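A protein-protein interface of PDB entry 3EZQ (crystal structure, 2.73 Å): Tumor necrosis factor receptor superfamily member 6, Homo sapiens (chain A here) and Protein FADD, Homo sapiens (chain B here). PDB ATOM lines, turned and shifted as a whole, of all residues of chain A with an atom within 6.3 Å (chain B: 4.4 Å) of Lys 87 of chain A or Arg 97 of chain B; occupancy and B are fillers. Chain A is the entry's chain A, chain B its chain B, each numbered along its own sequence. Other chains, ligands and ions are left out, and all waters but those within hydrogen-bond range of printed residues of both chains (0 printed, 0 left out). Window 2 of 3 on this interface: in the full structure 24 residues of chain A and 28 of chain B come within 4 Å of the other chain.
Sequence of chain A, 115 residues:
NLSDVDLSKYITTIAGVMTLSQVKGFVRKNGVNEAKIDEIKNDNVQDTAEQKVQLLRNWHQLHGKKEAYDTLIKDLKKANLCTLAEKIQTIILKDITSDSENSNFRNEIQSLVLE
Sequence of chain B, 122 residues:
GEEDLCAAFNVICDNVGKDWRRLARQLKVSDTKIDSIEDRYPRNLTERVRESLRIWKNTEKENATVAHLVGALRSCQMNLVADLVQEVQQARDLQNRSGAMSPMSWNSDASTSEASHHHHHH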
ATOM      1  N   CYS A  82      20.439   5.651  -2.634  1.00  0.00           N
ATOM      2  CA  CYS A  82      20.729   5.261  -4.025  1.00  0.00           C
ATOM      3  C   CYS A  82      21.619   6.276  -4.756  1.00  0.00           C
ATOM      4  O   CYS A  82      22.552   5.889  -5.455  1.00  0.00           O
ATOM      5  CB  CYS A  82      19.472   5.038  -4.827  1.00  0.00           C
ATOM      6  SG  CYS A  82      18.353   3.753  -4.212  1.00  0.00           S
ATOM      7  N   THR A  83      21.378   7.571  -4.591  1.00  0.00           N
ATOM      8  CA  THR A  83      22.171   8.523  -5.321  1.00  0.00           C
ATOM      9  C   THR A  83      23.606   8.526  -4.796  1.00  0.00           C
ATOM     10  O   THR A  83      24.540   8.608  -5.589  1.00  0.00           O
ATOM     11  CB  THR A  83      21.499   9.894  -5.308  1.00  0.00           C
ATOM     12  OG1 THR A  83      20.276   9.760  -6.025  1.00  0.00           O
ATOM     13  CG2 THR A  83      22.374  10.938  -5.973  1.00  0.00           C
ATOM     14  N   LEU A  84      23.776   8.427  -3.479  1.00  0.00           N
ATOM     15  CA  LEU A  84      25.109   8.311  -2.900  1.00  0.00           C
ATOM     16  C   LEU A  84      25.860   7.110  -3.464  1.00  0.00           C
ATOM     17  O   LEU A  84      27.022   7.208  -3.817  1.00  0.00           O
ATOM     18  CB  LEU A  84      25.008   8.122  -1.409  1.00  0.00           C
ATOM     19  CG  LEU A  84      24.954   9.378  -0.570  1.00  0.00           C
ATOM     20  CD1 LEU A  84      24.416   8.980   0.795  1.00  0.00           C
ATOM     21  CD2 LEU A  84      26.334  10.001  -0.466  1.00  0.00           C
ATOM     22  N   ALA A  85      25.181   5.974  -3.526  1.00  0.00           N
ATOM     23  CA  ALA A  85      25.766   4.767  -4.036  1.00  0.00           C
ATOM     24  C   ALA A  85      26.208   5.001  -5.488  1.00  0.00           C
ATOM     25  O   ALA A  85      27.279   4.568  -5.898  1.00  0.00           O
ATOM     26  CB  ALA A  85      24.756   3.628  -3.921  1.00  0.00           C
ATOM     27  N   GLU A  86      25.416   5.722  -6.278  1.00  0.00           N
ATOM     28  CA  GLU A  86      25.761   5.876  -7.703  1.00  0.00           C
ATOM     29  C   GLU A  86      26.942   6.827  -7.837  1.00  0.00           C
ATOM     30  O   GLU A  86      27.931   6.558  -8.559  1.00  0.00           O
ATOM     31  CB  GLU A  86      24.531   6.304  -8.482  1.00  0.00           C
ATOM     32  CG  GLU A  86      23.482   5.155  -8.493  1.00  0.00           C
ATOM     33  CD  GLU A  86      22.030   5.573  -8.906  1.00  0.00           C
ATOM     34  OE1 GLU A  86      21.682   6.774  -8.797  1.00  0.00           O
ATOM     35  OE2 GLU A  86      21.234   4.679  -9.318  1.00  0.00           O
ATOM     36  N   LYS A  87      26.884   7.905  -7.076  1.00  0.00           N
ATOM     37  CA  LYS A  87      27.899   8.898  -7.167  1.00  0.00           C
ATOM     38  C   LYS A  87      29.228   8.434  -6.588  1.00  0.00           C
ATOM     39  O   LYS A  87      30.277   8.722  -7.177  1.00  0.00           O
ATOM     40  CB  LYS A  87      27.389  10.181  -6.559  1.00  0.00           C
ATOM     41  CG  LYS A  87      26.448  10.870  -7.537  1.00  0.00           C
ATOM     42  CD  LYS A  87      25.922  12.155  -6.957  1.00  0.00           C
ATOM     43  CE  LYS A  87      24.884  12.785  -7.840  1.00  0.00           C
ATOM     44  NZ  LYS A  87      25.355  13.005  -9.261  1.00  0.00           N
ATOM     45  N   ILE A  88      29.200   7.674  -5.493  1.00  0.00           N
ATOM     46  CA  ILE A  88      30.433   7.164  -4.926  1.00  0.00           C
ATOM     47  C   ILE A  88      31.008   6.073  -5.822  1.00  0.00           C
ATOM     48  O   ILE A  88      32.226   6.028  -6.050  1.00  0.00           O
ATOM     49  CB  ILE A  88      30.288   6.665  -3.482  1.00  0.00           C
ATOM     50  CG1 ILE A  88      29.846   7.827  -2.560  1.00  0.00           C
ATOM     51  CG2 ILE A  88      31.618   6.078  -3.017  1.00  0.00           C
ATOM     52  CD1 ILE A  88      29.257   7.358  -1.204  1.00  0.00           C
ATOM     53  N   GLN A  89      30.157   5.232  -6.397  1.00  0.00           N
ATOM     54  CA  GLN A  89      30.691   4.241  -7.340  1.00  0.00           C
ATOM     55  C   GLN A  89      31.403   4.878  -8.513  1.00  0.00           C
ATOM     56  O   GLN A  89      32.438   4.395  -8.943  1.00  0.00           O
ATOM     57  CB  GLN A  89      29.617   3.350  -7.880  1.00  0.00           C
ATOM     58  CG  GLN A  89      30.169   2.352  -8.829  1.00  0.00           C
ATOM     59  CD  GLN A  89      29.182   1.245  -9.129  1.00  0.00           C
ATOM     60  OE1 GLN A  89      28.243   1.411  -9.941  1.00  0.00           O
ATOM     61  NE2 GLN A  89      29.380   0.108  -8.472  1.00  0.00           N
ATOM     62  N   THR A  90      30.851   5.962  -9.039  1.00  0.00           N
ATOM     63  CA  THR A  90      31.480   6.630 -10.132  1.00  0.00           C
ATOM     64  C   THR A  90      32.864   7.174  -9.762  1.00  0.00           C
ATOM     65  O   THR A  90      33.808   7.028 -10.535  1.00  0.00           O
ATOM     66  CB  THR A  90      30.623   7.846 -10.602  1.00  0.00           C
ATOM     67  OG1 THR A  90      29.338   7.402 -11.023  1.00  0.00           O
ATOM     68  CG2 THR A  90      31.337   8.613 -11.712  1.00  0.00           C
ATOM     69  N   ILE A  91      32.973   7.825  -8.610  1.00  0.00           N
ATOM     70  CA  ILE A  91      34.273   8.328  -8.154  1.00  0.00           C
ATOM     71  C   ILE A  91      35.292   7.188  -8.034  1.00  0.00           C
ATOM     72  O   ILE A  91      36.370   7.263  -8.589  1.00  0.00           O
ATOM     73  CB  ILE A  91      34.102   9.054  -6.793  1.00  0.00           C
ATOM     74  CG1 ILE A  91      33.393  10.407  -7.004  1.00  0.00           C
ATOM     75  CG2 ILE A  91      35.469   9.215  -6.084  1.00  0.00           C
ATOM     76  CD1 ILE A  91      32.420  10.789  -5.870  1.00  0.00           C
ATOM     77  N   ILE A  92      34.903   6.126  -7.353  1.00  0.00           N
ATOM     78  CA  ILE A  92      35.775   4.979  -7.126  1.00  0.00           C
ATOM     79  C   ILE A  92      36.245   4.335  -8.427  1.00  0.00           C
ATOM     80  O   ILE A  92      37.453   4.162  -8.607  1.00  0.00           O
ATOM     81  CB  ILE A  92      35.119   3.926  -6.216  1.00  0.00           C
ATOM     82  CG1 ILE A  92      34.942   4.542  -4.819  1.00  0.00           C
ATOM     83  CG2 ILE A  92      35.975   2.688  -6.212  1.00  0.00           C
ATOM     84  CD1 ILE A  92      34.358   3.674  -3.778  1.00  0.00           C
ATOM     85  N   LEU A 112      29.883  15.227  -0.864  1.00  0.00           N
ATOM     86  CA  LEU A 112      28.621  14.505  -1.043  1.00  0.00           C
ATOM     87  C   LEU A 112      27.843  14.417   0.268  1.00  0.00           C
ATOM     88  O   LEU A 112      26.641  14.197   0.263  1.00  0.00           O
ATOM     89  CB  LEU A 112      28.857  13.075  -1.564  1.00  0.00           C
ATOM     90  CG  LEU A 112      29.312  12.967  -3.026  1.00  0.00           C
ATOM     91  CD1 LEU A 112      29.639  11.545  -3.386  1.00  0.00           C
ATOM     92  CD2 LEU A 112      28.250  13.549  -3.995  1.00  0.00           C
ATOM     93  N   LEU B  94      23.434  16.093  -2.995  1.00  0.00           N
ATOM     94  CA  LEU B  94      23.532  15.184  -4.117  1.00  0.00           C
ATOM     95  C   LEU B  94      23.082  15.814  -5.417  1.00  0.00           C
ATOM     96  O   LEU B  94      23.231  15.219  -6.480  1.00  0.00           O
ATOM     97  CB  LEU B  94      22.696  13.931  -3.821  1.00  0.00           C
ATOM     98  CG  LEU B  94      23.212  13.090  -2.666  1.00  0.00           C
ATOM     99  CD1 LEU B  94      22.211  12.002  -2.361  1.00  0.00           C
ATOM    100  CD2 LEU B  94      24.622  12.518  -3.022  1.00  0.00           C
ATOM    101  N   GLN B  95      22.525  17.014  -5.336  1.00  0.00           N
ATOM    102  CA  GLN B  95      22.100  17.731  -6.539  1.00  0.00           C
ATOM    103  C   GLN B  95      23.182  18.648  -7.066  1.00  0.00           C
ATOM    104  O   GLN B  95      23.351  18.750  -8.276  1.00  0.00           O
ATOM    105  CB  GLN B  95      20.840  18.532  -6.277  1.00  0.00           C
ATOM    106  CG  GLN B  95      19.685  17.649  -5.928  1.00  0.00           C
ATOM    107  CD  GLN B  95      18.414  18.408  -5.894  1.00  0.00           C
ATOM    108  OE1 GLN B  95      18.349  19.490  -5.315  1.00  0.00           O
ATOM    109  NE2 GLN B  95      17.380  17.861  -6.527  1.00  0.00           N
ATOM    110  N   ASN B  96      23.919  19.303  -6.168  1.00  0.00           N
ATOM    111  CA  ASN B  96      25.035  20.170  -6.577  1.00  0.00           C
ATOM    112  C   ASN B  96      25.917  19.538  -7.680  1.00  0.00           C
ATOM    113  O   ASN B  96      26.326  20.218  -8.639  1.00  0.00           O
ATOM    114  CB  ASN B  96      25.899  20.573  -5.365  1.00  0.00           C
ATOM    115  CG  ASN B  96      26.832  21.764  -5.667  1.00  0.00           C
ATOM    116  OD1 ASN B  96      26.374  22.857  -6.013  1.00  0.00           O
ATOM    117  ND2 ASN B  96      28.140  21.548  -5.529  1.00  0.00           N
ATOM    118  N   ARG B  97      26.186  18.239  -7.538  1.00  0.00           N
ATOM    119  CA  ARG B  97      26.987  17.476  -8.502  1.00  0.00           C
ATOM    120  C   ARG B  97      26.231  17.218  -9.832  1.00  0.00           C
ATOM    121  O   ARG B  97      26.751  17.493 -10.921  1.00  0.00           O
ATOM    122  CB  ARG B  97      27.427  16.151  -7.843  1.00  0.00           C
ATOM    123  CG  ARG B  97      28.490  15.410  -8.623  1.00  0.00           C
ATOM    124  CD  ARG B  97      27.864  14.544  -9.691  1.00  0.00           C
ATOM    125  NE  ARG B  97      28.732  14.346 -10.848  1.00  0.00           N
ATOM    126  CZ  ARG B  97      29.079  13.156 -11.341  1.00  0.00           C
ATOM    127  NH1 ARG B  97      28.624  12.031 -10.796  1.00  0.00           N
ATOM    128  NH2 ARG B  97      29.890  13.087 -12.398  1.00  0.00           N
ATOM    129  N   SER B  98      25.016  16.675  -9.732  1.00  0.00           N
ATOM    130  CA  SER B  98      24.205  16.365 -10.919  1.00  0.00           C
ATOM    131  C   SER B  98      23.577  17.651 -11.486  1.00  0.00           C
ATOM    132  O   SER B  98      23.706  17.929 -12.684  1.00  0.00           O
ATOM    133  CB  SER B  98      23.132  15.306 -10.619  1.00  0.00           C
ATOM    134  OG  SER B  98      22.889  14.495 -11.765  1.00  0.00           O
ATOM    135  N   GLY B  99      22.920  18.432 -10.620  1.00  0.00           N
ATOM    136  CA  GLY B  99      22.322  19.722 -11.004  1.00  0.00           C
ATOM    137  C   GLY B  99      23.120  20.940 -10.552  1.00  0.00           C
ATOM    138  O   GLY B  99      23.169  21.271  -9.362  1.00  0.00           O
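Among the printed residues, pairs that only touch across the chains: Lys 87 of chain A with Arg 97 of chain B (3.0 Å), Lys 87 of chain A with Leu 94 of chain B (3.2 Å), Lys 87 of chain A with Ser 98 of chain B (3.5 Å), Thr 83 of chain A with Leu 94 of chain B (3.7 Å), Leu 112 of chain A with Leu 94 of chain B (3.9 Å) and Leu 84 of chain A with Leu 94 of chain B (3.97 Å).
Of the printed residues of chain B, Thr 83 of chain A touches Leu 94 (3.7 Å). Of the printed residues of chain B, Leu 84 of chain A touches Leu 94. Of chain B, only Leu 94, Arg 97 and Ser 98 come within 4 Å of Lys 87 of chain A. Ile 88 of chain A touches none of the printed residues of chain B. Asn 96 of chain B touches none of the printed residues of chain A. The nearest residue of chain A that does not touch Arg 97 of chain B is Thr 90 of chain A (4.5 Å).
Hydrophobic or aromatic side chains of chain B within 4 Å of the printed part of chain A: Leu 94. Along chain B the printed residues that touch a printed residue of chain A span positions 94 to 98. Printed residues of chain A that touch a printed residue of chain B: Thr 83, Leu 84, Lys 87 and Leu 112. Among the printed residues, no Asp or Glu carboxylate lies within 4 Å of a Lys or Arg side-chain nitrogen of the other chain.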
